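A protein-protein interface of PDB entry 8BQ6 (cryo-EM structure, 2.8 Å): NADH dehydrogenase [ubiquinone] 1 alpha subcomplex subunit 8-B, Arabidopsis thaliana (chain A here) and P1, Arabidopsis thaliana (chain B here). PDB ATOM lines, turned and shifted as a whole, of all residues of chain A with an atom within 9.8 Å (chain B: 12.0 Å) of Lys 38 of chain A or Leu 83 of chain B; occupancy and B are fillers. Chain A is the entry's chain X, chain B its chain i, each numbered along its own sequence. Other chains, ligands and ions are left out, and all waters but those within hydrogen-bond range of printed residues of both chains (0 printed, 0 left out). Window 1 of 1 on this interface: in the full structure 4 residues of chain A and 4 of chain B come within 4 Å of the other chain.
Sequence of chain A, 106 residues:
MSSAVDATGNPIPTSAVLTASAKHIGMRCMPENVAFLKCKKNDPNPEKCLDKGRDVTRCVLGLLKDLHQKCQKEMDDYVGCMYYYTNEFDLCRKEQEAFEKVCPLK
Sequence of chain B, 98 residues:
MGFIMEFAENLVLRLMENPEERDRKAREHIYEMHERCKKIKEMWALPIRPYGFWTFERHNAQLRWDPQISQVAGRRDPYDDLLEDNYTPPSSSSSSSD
No residue of chain B comes within 4 Å of Val 34 of chain A. No residue of chain B comes within 4 Å of Ala 35 of chain A. Leu 37 of chain A touches two residues of chain B. Lys 38 of chain A touches one residue of chain B. Of chain B, only Asp 80 (3.1 Å) and Leu 83 (3.5 Å) come within 4 Å of Lys 41 of chain A. Asp 43 of chain A touches none of the printed residues of chain B. Gln 71 of chain B touches none of the printed residues of chain A. Of the printed residues of chain A, Tyr 79 of chain B touches Lys 40 (3.2 Å). Of the printed residues of chain A, Asp 80 of chain B touches Lys 41. Of chain A, only Leu 37 (3.6 Å) comes within 4 Å of Leu 82 of chain B. Leu 83 of chain B touches just these residues of chain A: Leu 37, Lys 38 and Lys 41. Glu 84 of chain B touches none of the printed residues of chain A. The nearest residue of chain B that does not touch Lys 38 of chain A is Tyr 79 of chain B (6.6 Å). The nearest residue of chain A that does not touch Leu 83 of chain B is Val 34 of chain A (4.2 Å). The nearest printed residue of chain A that does not touch Tyr 79 of chain B is Lys 41 of chain A (4.3 Å).
Of the 10 printed residues of chain B, 4 touch a printed residue of chain A. Hydrophobic or aromatic side chains of chain B within 4 Å of the printed part of chain A: Tyr 79, Leu 82 and Leu 83. Among the printed residues, Asp or Glu carboxylates within 4 Å of a Lys or Arg side-chain nitrogen of the other chain: Lys 41 of chain A with Asp 80 of chain B.
N of Asp 77 of chain B lies close to OD2 of Asp 80 of chain B, at 3.3 Å.
The side-chain amino group of Lys 41 of chain A is in salt-bridge range of the side-chain carboxylate of Asp 80 of chain B (3.4 Å).
Among the printed residues, pairs that only touch across the chains: Leu 37 of chain A with Leu 82 of chain B, Leu 37 of chain A with Leu 83 of chain B, Lys 38 of chain A with Leu 83 of chain B, Lys 40 of chain A with Tyr 79 of chain B and Lys 41 of chain A with Leu 83 of chain B.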
ATOM      1  N   MET A  30     -32.146  35.609  -4.318  1.00  0.00           N
ATOM      2  CA  MET A  30     -31.008  35.432  -5.215  1.00  0.00           C
ATOM      3  C   MET A  30     -29.663  35.675  -4.541  1.00  0.00           C
ATOM      4  O   MET A  30     -28.763  34.833  -4.700  1.00  0.00           O
ATOM      5  CB  MET A  30     -31.188  36.341  -6.436  1.00  0.00           C
ATOM      6  CG  MET A  30     -29.972  36.431  -7.337  1.00  0.00           C
ATOM      7  SD  MET A  30     -29.602  34.870  -8.154  1.00  0.00           S
ATOM      8  CE  MET A  30     -31.044  34.697  -9.200  1.00  0.00           C
ATOM      9  N   PRO A  31     -29.448  36.762  -3.782  1.00  0.00           N
ATOM     10  CA  PRO A  31     -28.093  36.996  -3.248  1.00  0.00           C
ATOM     11  C   PRO A  31     -27.630  35.945  -2.255  1.00  0.00           C
ATOM     12  O   PRO A  31     -26.473  35.509  -2.321  1.00  0.00           O
ATOM     13  CB  PRO A  31     -28.206  38.381  -2.592  1.00  0.00           C
ATOM     14  CG  PRO A  31     -29.453  38.983  -3.130  1.00  0.00           C
ATOM     15  CD  PRO A  31     -30.370  37.841  -3.386  1.00  0.00           C
ATOM     16  N   GLU A  32     -28.491  35.535  -1.319  1.00  0.00           N
ATOM     17  CA  GLU A  32     -28.088  34.526  -0.345  1.00  0.00           C
ATOM     18  C   GLU A  32     -27.806  33.191  -1.024  1.00  0.00           C
ATOM     19  O   GLU A  32     -26.847  32.492  -0.668  1.00  0.00           O
ATOM     20  CB  GLU A  32     -29.166  34.370   0.728  1.00  0.00           C
ATOM     21  CG  GLU A  32     -29.282  35.547   1.686  1.00  0.00           C
ATOM     22  CD  GLU A  32     -30.273  36.594   1.215  1.00  0.00           C
ATOM     23  OE1 GLU A  32     -30.873  36.406   0.137  1.00  0.00           O
ATOM     24  OE2 GLU A  32     -30.459  37.602   1.928  1.00  0.00           O
ATOM     25  N   ASN A  33     -28.631  32.827  -2.010  1.00  0.00           N
ATOM     26  CA  ASN A  33     -28.382  31.626  -2.799  1.00  0.00           C
ATOM     27  C   ASN A  33     -27.025  31.694  -3.487  1.00  0.00           C
ATOM     28  O   ASN A  33     -26.258  30.725  -3.473  1.00  0.00           O
ATOM     29  CB  ASN A  33     -29.486  31.443  -3.843  1.00  0.00           C
ATOM     30  CG  ASN A  33     -30.751  30.830  -3.271  1.00  0.00           C
ATOM     31  OD1 ASN A  33     -30.820  30.492  -2.090  1.00  0.00           O
ATOM     32  ND2 ASN A  33     -31.762  30.684  -4.116  1.00  0.00           N
ATOM     33  N   VAL A  34     -26.717  32.836  -4.108  1.00  0.00           N
ATOM     34  CA  VAL A  34     -25.460  32.959  -4.839  1.00  0.00           C
ATOM     35  C   VAL A  34     -24.276  32.863  -3.887  1.00  0.00           C
ATOM     36  O   VAL A  34     -23.272  32.210  -4.190  1.00  0.00           O
ATOM     37  CB  VAL A  34     -25.433  34.264  -5.656  1.00  0.00           C
ATOM     38  CG1 VAL A  34     -24.036  34.527  -6.201  1.00  0.00           C
ATOM     39  CG2 VAL A  34     -26.424  34.183  -6.795  1.00  0.00           C
ATOM     40  N   ALA A  35     -24.373  33.508  -2.722  1.00  0.00           N
ATOM     41  CA  ALA A  35     -23.281  33.455  -1.752  1.00  0.00           C
ATOM     42  C   ALA A  35     -23.055  32.032  -1.255  1.00  0.00           C
ATOM     43  O   ALA A  35     -21.911  31.559  -1.164  1.00  0.00           O
ATOM     44  CB  ALA A  35     -23.578  34.390  -0.581  1.00  0.00           C
ATOM     45  N   PHE A  36     -24.147  31.338  -0.923  1.00  0.00           N
ATOM     46  CA  PHE A  36     -24.054  29.941  -0.526  1.00  0.00           C
ATOM     47  C   PHE A  36     -23.379  29.102  -1.602  1.00  0.00           C
ATOM     48  O   PHE A  36     -22.459  28.332  -1.308  1.00  0.00           O
ATOM     49  CB  PHE A  36     -25.451  29.403  -0.232  1.00  0.00           C
ATOM     50  CG  PHE A  36     -25.466  27.990   0.244  1.00  0.00           C
ATOM     51  CD1 PHE A  36     -25.191  27.688   1.560  1.00  0.00           C
ATOM     52  CD2 PHE A  36     -25.750  26.957  -0.631  1.00  0.00           C
ATOM     53  CE1 PHE A  36     -25.209  26.387   1.997  1.00  0.00           C
ATOM     54  CE2 PHE A  36     -25.764  25.655  -0.198  1.00  0.00           C
ATOM     55  CZ  PHE A  36     -25.491  25.369   1.119  1.00  0.00           C
ATOM     56  N   LEU A  37     -23.827  29.233  -2.853  1.00  0.00           N
ATOM     57  CA  LEU A  37     -23.277  28.404  -3.920  1.00  0.00           C
ATOM     58  C   LEU A  37     -21.809  28.724  -4.170  1.00  0.00           C
ATOM     59  O   LEU A  37     -21.007  27.820  -4.430  1.00  0.00           O
ATOM     60  CB  LEU A  37     -24.101  28.577  -5.194  1.00  0.00           C
ATOM     61  CG  LEU A  37     -25.533  28.054  -5.079  1.00  0.00           C
ATOM     62  CD1 LEU A  37     -26.306  28.261  -6.368  1.00  0.00           C
ATOM     63  CD2 LEU A  37     -25.520  26.589  -4.685  1.00  0.00           C
ATOM     64  N   LYS A  38     -21.434  30.001  -4.081  1.00  0.00           N
ATOM     65  CA  LYS A  38     -20.038  30.377  -4.262  1.00  0.00           C
ATOM     66  C   LYS A  38     -19.159  29.738  -3.195  1.00  0.00           C
ATOM     67  O   LYS A  38     -18.115  29.144  -3.498  1.00  0.00           O
ATOM     68  CB  LYS A  38     -19.905  31.899  -4.234  1.00  0.00           C
ATOM     69  CG  LYS A  38     -18.590  32.409  -4.777  1.00  0.00           C
ATOM     70  CD  LYS A  38     -18.802  33.440  -5.873  1.00  0.00           C
ATOM     71  CE  LYS A  38     -19.996  34.342  -5.589  1.00  0.00           C
ATOM     72  NZ  LYS A  38     -20.116  35.423  -6.606  1.00  0.00           N
ATOM     73  N   CYS A  39     -19.582  29.825  -1.934  1.00  0.00           N
ATOM     74  CA  CYS A  39     -18.749  29.260  -0.880  1.00  0.00           C
ATOM     75  C   CYS A  39     -18.787  27.733  -0.896  1.00  0.00           C
ATOM     76  O   CYS A  39     -17.828  27.083  -0.465  1.00  0.00           O
ATOM     77  CB  CYS A  39     -19.165  29.836   0.470  1.00  0.00           C
ATOM     78  SG  CYS A  39     -20.875  29.639   0.866  1.00  0.00           S
ATOM     79  N   LYS A  40     -19.869  27.138  -1.413  1.00  0.00           N
ATOM     80  CA  LYS A  40     -19.871  25.695  -1.642  1.00  0.00           C
ATOM     81  C   LYS A  40     -18.852  25.315  -2.707  1.00  0.00           C
ATOM     82  O   LYS A  40     -18.155  24.302  -2.581  1.00  0.00           O
ATOM     83  CB  LYS A  40     -21.265  25.210  -2.047  1.00  0.00           C
ATOM     84  CG  LYS A  40     -22.202  24.972  -0.883  1.00  0.00           C
ATOM     85  CD  LYS A  40     -21.513  24.162   0.193  1.00  0.00           C
ATOM     86  CE  LYS A  40     -21.528  22.685  -0.108  1.00  0.00           C
ATOM     87  NZ  LYS A  40     -21.761  21.904   1.134  1.00  0.00           N
ATOM     88  N   LYS A  41     -18.759  26.120  -3.766  1.00  0.00           N
ATOM     89  CA  LYS A  41     -17.747  25.894  -4.790  1.00  0.00           C
ATOM     90  C   LYS A  41     -16.343  25.961  -4.205  1.00  0.00           C
ATOM     91  O   LYS A  41     -15.493  25.118  -4.514  1.00  0.00           O
ATOM     92  CB  LYS A  41     -17.904  26.920  -5.909  1.00  0.00           C
ATOM     93  CG  LYS A  41     -17.264  26.521  -7.217  1.00  0.00           C
ATOM     94  CD  LYS A  41     -17.469  27.606  -8.252  1.00  0.00           C
ATOM     95  CE  LYS A  41     -16.968  27.186  -9.613  1.00  0.00           C
ATOM     96  NZ  LYS A  41     -16.747  28.353 -10.509  1.00  0.00           N
ATOM     97  N   ASN A  42     -16.076  26.962  -3.361  1.00  0.00           N
ATOM     98  CA  ASN A  42     -14.745  27.076  -2.766  1.00  0.00           C
ATOM     99  C   ASN A  42     -14.459  25.925  -1.805  1.00  0.00           C
ATOM    100  O   ASN A  42     -13.362  25.354  -1.824  1.00  0.00           O
ATOM    101  CB  ASN A  42     -14.597  28.422  -2.053  1.00  0.00           C
ATOM    102  CG  ASN A  42     -13.155  28.730  -1.664  1.00  0.00           C
ATOM    103  OD1 ASN A  42     -12.486  27.929  -1.010  1.00  0.00           O
ATOM    104  ND2 ASN A  42     -12.673  29.897  -2.070  1.00  0.00           N
ATOM    105  N   ASP A  43     -15.421  25.572  -0.957  1.00  0.00           N
ATOM    106  CA  ASP A  43     -15.153  24.543   0.038  1.00  0.00           C
ATOM    107  C   ASP A  43     -16.341  23.606   0.212  1.00  0.00           C
ATOM    108  O   ASP A  43     -17.400  24.021   0.699  1.00  0.00           O
ATOM    109  CB  ASP A  43     -14.781  25.179   1.377  1.00  0.00           C
ATOM    110  CG  ASP A  43     -13.602  24.497   2.030  1.00  0.00           C
ATOM    111  OD1 ASP A  43     -13.492  23.261   1.893  1.00  0.00           O
ATOM    112  OD2 ASP A  43     -12.780  25.191   2.664  1.00  0.00           O
ATOM    113  N   PRO A  44     -16.197  22.332  -0.163  1.00  0.00           N
ATOM    114  CA  PRO A  44     -17.306  21.382  -0.011  1.00  0.00           C
ATOM    115  C   PRO A  44     -17.575  20.960   1.421  1.00  0.00           C
ATOM    116  O   PRO A  44     -18.562  20.253   1.658  1.00  0.00           O
ATOM    117  CB  PRO A  44     -16.836  20.189  -0.847  1.00  0.00           C
ATOM    118  CG  PRO A  44     -15.352  20.223  -0.642  1.00  0.00           C
ATOM    119  CD  PRO A  44     -15.031  21.690  -0.792  1.00  0.00           C
ATOM    120  N   LYS A  48     -17.843  24.364   7.139  1.00  0.00           N
ATOM    121  CA  LYS A  48     -17.318  25.656   6.710  1.00  0.00           C
ATOM    122  C   LYS A  48     -18.309  26.459   5.888  1.00  0.00           C
ATOM    123  O   LYS A  48     -17.899  27.342   5.127  1.00  0.00           O
ATOM    124  CB  LYS A  48     -16.033  25.458   5.905  1.00  0.00           C
ATOM    125  CG  LYS A  48     -14.996  24.615   6.607  1.00  0.00           C
ATOM    126  CD  LYS A  48     -14.662  25.207   7.963  1.00  0.00           C
ATOM    127  CE  LYS A  48     -13.508  24.474   8.618  1.00  0.00           C
ATOM    128  NZ  LYS A  48     -13.937  23.197   9.246  1.00  0.00           N
ATOM    129  N   CYS A  49     -19.612  26.179   5.988  1.00  0.00           N
ATOM    130  CA  CYS A  49     -20.620  27.020   5.264  1.00  0.00           C
ATOM    131  C   CYS A  49     -21.927  27.146   6.046  1.00  0.00           C
ATOM    132  O   CYS A  49     -22.896  27.668   5.467  1.00  0.00           O
ATOM    133  CB  CYS A  49     -21.012  26.454   3.902  1.00  0.00           C
ATOM    134  SG  CYS A  49     -19.686  26.401   2.671  1.00  0.00           S
ATOM    135  N   LYS A  52     -23.402  30.882   5.876  1.00  0.00           N
ATOM    136  CA  LYS A  52     -24.061  31.218   4.587  1.00  0.00           C
ATOM    137  C   LYS A  52     -25.362  30.422   4.467  1.00  0.00           C
ATOM    138  O   LYS A  52     -26.324  30.963   3.911  1.00  0.00           O
ATOM    139  CB  LYS A  52     -23.116  30.939   3.414  1.00  0.00           C
ATOM    140  CG  LYS A  52     -22.458  32.171   2.814  1.00  0.00           C
ATOM    141  CD  LYS A  52     -21.287  32.664   3.636  1.00  0.00           C
ATOM    142  CE  LYS A  52     -20.517  33.782   2.973  1.00  0.00           C
ATOM    143  NZ  LYS A  52     -19.881  33.338   1.711  1.00  0.00           N
ATOM    144  N   VAL A  56     -29.417  31.657   3.985  1.00  0.00           N
ATOM    145  CA  VAL A  56     -30.361  31.132   2.999  1.00  0.00           C
ATOM    146  C   VAL A  56     -31.642  30.678   3.686  1.00  0.00           C
ATOM    147  O   VAL A  56     -32.756  30.973   3.231  1.00  0.00           O
ATOM    148  CB  VAL A  56     -29.717  29.993   2.187  1.00  0.00           C
ATOM    149  CG1 VAL A  56     -30.779  29.055   1.642  1.00  0.00           C
ATOM    150  CG2 VAL A  56     -28.903  30.560   1.050  1.00  0.00           C
ATOM    151  N   GLN B  71     -14.556  22.480 -19.228  1.00  0.00           N
ATOM    152  CA  GLN B  71     -15.914  23.006 -19.191  1.00  0.00           C
ATOM    153  C   GLN B  71     -16.912  22.138 -19.950  1.00  0.00           C
ATOM    154  O   GLN B  71     -18.056  22.556 -20.144  1.00  0.00           O
ATOM    155  CB  GLN B  71     -15.942  24.426 -19.759  1.00  0.00           C
ATOM    156  CG  GLN B  71     -16.011  25.527 -18.728  1.00  0.00           C
ATOM    157  CD  GLN B  71     -15.113  25.273 -17.544  1.00  0.00           C
ATOM    158  OE1 GLN B  71     -15.571  24.864 -16.480  1.00  0.00           O
ATOM    159  NE2 GLN B  71     -13.820  25.507 -17.723  1.00  0.00           N
ATOM    160  N   ARG B  76     -17.736  18.163 -15.583  1.00  0.00           N
ATOM    161  CA  ARG B  76     -17.703  19.392 -14.808  1.00  0.00           C
ATOM    162  C   ARG B  76     -17.971  19.124 -13.337  1.00  0.00           C
ATOM    163  O   ARG B  76     -18.679  18.182 -12.971  1.00  0.00           O
ATOM    164  CB  ARG B  76     -18.734  20.384 -15.331  1.00  0.00           C
ATOM    165  CG  ARG B  76     -18.670  20.539 -16.814  1.00  0.00           C
ATOM    166  CD  ARG B  76     -19.487  21.696 -17.278  1.00  0.00           C
ATOM    167  NE  ARG B  76     -18.966  22.963 -16.787  1.00  0.00           N
ATOM    168  CZ  ARG B  76     -19.626  24.109 -16.871  1.00  0.00           C
ATOM    169  NH1 ARG B  76     -20.810  24.180 -17.454  1.00  0.00           N
ATOM    170  NH2 ARG B  76     -19.081  25.211 -16.367  1.00  0.00           N
ATOM    171  N   ASP B  77     -17.394  19.970 -12.498  1.00  0.00           N
ATOM    172  CA  ASP B  77     -17.830  20.054 -11.116  1.00  0.00           C
ATOM    173  C   ASP B  77     -19.311  20.418 -11.101  1.00  0.00           C
ATOM    174  O   ASP B  77     -19.731  21.309 -11.852  1.00  0.00           O
ATOM    175  CB  ASP B  77     -16.992  21.097 -10.373  1.00  0.00           C
ATOM    176  CG  ASP B  77     -17.315  21.186  -8.890  1.00  0.00           C
ATOM    177  OD1 ASP B  77     -18.178  20.435  -8.392  1.00  0.00           O
ATOM    178  OD2 ASP B  77     -16.684  22.021  -8.210  1.00  0.00           O
ATOM    179  N   PRO B  78     -20.137  19.732 -10.308  1.00  0.00           N
ATOM    180  CA  PRO B  78     -21.583  20.011 -10.342  1.00  0.00           C
ATOM    181  C   PRO B  78     -21.957  21.441  -9.985  1.00  0.00           C
ATOM    182  O   PRO B  78     -22.981  21.934 -10.471  1.00  0.00           O
ATOM    183  CB  PRO B  78     -22.155  19.003  -9.334  1.00  0.00           C
ATOM    184  CG  PRO B  78     -20.979  18.522  -8.536  1.00  0.00           C
ATOM    185  CD  PRO B  78     -19.826  18.561  -9.476  1.00  0.00           C
ATOM    186  N   TYR B  79     -21.170  22.126  -9.155  1.00  0.00           N
ATOM    187  CA  TYR B  79     -21.525  23.490  -8.779  1.00  0.00           C
ATOM    188  C   TYR B  79     -21.349  24.479  -9.923  1.00  0.00           C
ATOM    189  O   TYR B  79     -21.900  25.583  -9.857  1.00  0.00           O
ATOM    190  CB  TYR B  79     -20.708  23.923  -7.562  1.00  0.00           C
ATOM    191  CG  TYR B  79     -21.223  23.288  -6.297  1.00  0.00           C
ATOM    192  CD1 TYR B  79     -22.449  23.662  -5.771  1.00  0.00           C
ATOM    193  CD2 TYR B  79     -20.512  22.284  -5.656  1.00  0.00           C
ATOM    194  CE1 TYR B  79     -22.941  23.078  -4.631  1.00  0.00           C
ATOM    195  CE2 TYR B  79     -21.001  21.690  -4.510  1.00  0.00           C
ATOM    196  CZ  TYR B  79     -22.217  22.094  -4.003  1.00  0.00           C
ATOM    197  OH  TYR B  79     -22.721  21.516  -2.864  1.00  0.00           O
ATOM    198  N   ASP B  80     -20.615  24.104 -10.972  1.00  0.00           N
ATOM    199  CA  ASP B  80     -20.378  25.021 -12.082  1.00  0.00           C
ATOM    200  C   ASP B  80     -21.663  25.388 -12.805  1.00  0.00           C
ATOM    201  O   ASP B  80     -21.784  26.499 -13.331  1.00  0.00           O
ATOM    202  CB  ASP B  80     -19.391  24.405 -13.067  1.00  0.00           C
ATOM    203  CG  ASP B  80     -17.989  24.348 -12.517  1.00  0.00           C
ATOM    204  OD1 ASP B  80     -17.481  25.396 -12.077  1.00  0.00           O
ATOM    205  OD2 ASP B  80     -17.387  23.259 -12.540  1.00  0.00           O
ATOM    206  N   ASP B  81     -22.621  24.465 -12.865  1.00  0.00           N
ATOM    207  CA  ASP B  81     -23.881  24.766 -13.531  1.00  0.00           C
ATOM    208  C   ASP B  81     -24.726  25.722 -12.700  1.00  0.00           C
ATOM    209  O   ASP B  81     -25.515  26.501 -13.249  1.00  0.00           O
ATOM    210  CB  ASP B  81     -24.645  23.472 -13.802  1.00  0.00           C
ATOM    211  CG  ASP B  81     -24.428  22.957 -15.204  1.00  0.00           C
ATOM    212  OD1 ASP B  81     -25.065  21.947 -15.569  1.00  0.00           O
ATOM    213  OD2 ASP B  81     -23.621  23.562 -15.942  1.00  0.00           O
ATOM    214  N   LEU B  82     -24.576  25.676 -11.375  1.00  0.00           N
ATOM    215  CA  LEU B  82     -25.404  26.508 -10.511  1.00  0.00           C
ATOM    216  C   LEU B  82     -24.974  27.966 -10.541  1.00  0.00           C
ATOM    217  O   LEU B  82     -25.801  28.859 -10.322  1.00  0.00           O
ATOM    218  CB  LEU B  82     -25.376  25.983  -9.076  1.00  0.00           C
ATOM    219  CG  LEU B  82     -25.983  24.600  -8.819  1.00  0.00           C
ATOM    220  CD1 LEU B  82     -25.742  24.171  -7.379  1.00  0.00           C
ATOM    221  CD2 LEU B  82     -27.451  24.538  -9.171  1.00  0.00           C
ATOM    222  N   LEU B  83     -23.695  28.228 -10.796  1.00  0.00           N
ATOM    223  CA  LEU B  83     -23.172  29.584 -10.828  1.00  0.00           C
ATOM    224  C   LEU B  83     -23.064  30.147 -12.237  1.00  0.00           C
ATOM    225  O   LEU B  83     -22.927  31.365 -12.390  1.00  0.00           O
ATOM    226  CB  LEU B  83     -21.800  29.627 -10.148  1.00  0.00           C
ATOM    227  CG  LEU B  83     -21.866  29.355  -8.644  1.00  0.00           C
ATOM    228  CD1 LEU B  83     -20.488  29.269  -8.040  1.00  0.00           C
ATOM    229  CD2 LEU B  83     -22.666  30.441  -7.963  1.00  0.00           C
ATOM    230  N   GLU B  84     -23.143  29.302 -13.260  1.00  0.00           N
ATOM    231  CA  GLU B  84     -22.990  29.747 -14.638  1.00  0.00           C
ATOM    232  C   GLU B  84     -24.291  29.601 -15.419  1.00  0.00           C
ATOM    233  O   GLU B  84     -24.507  30.299 -16.410  1.00  0.00           O
ATOM    234  CB  GLU B  84     -21.874  28.962 -15.330  1.00  0.00           C
ATOM    235  CG  GLU B  84     -20.484  29.513 -15.077  1.00  0.00           C
ATOM    236  CD  GLU B  84     -20.224  30.806 -15.827  1.00  0.00           C
ATOM    237  OE1 GLU B  84     -20.747  30.963 -16.953  1.00  0.00           O
ATOM    238  OE2 GLU B  84     -19.490  31.663 -15.294  1.00  0.00           O
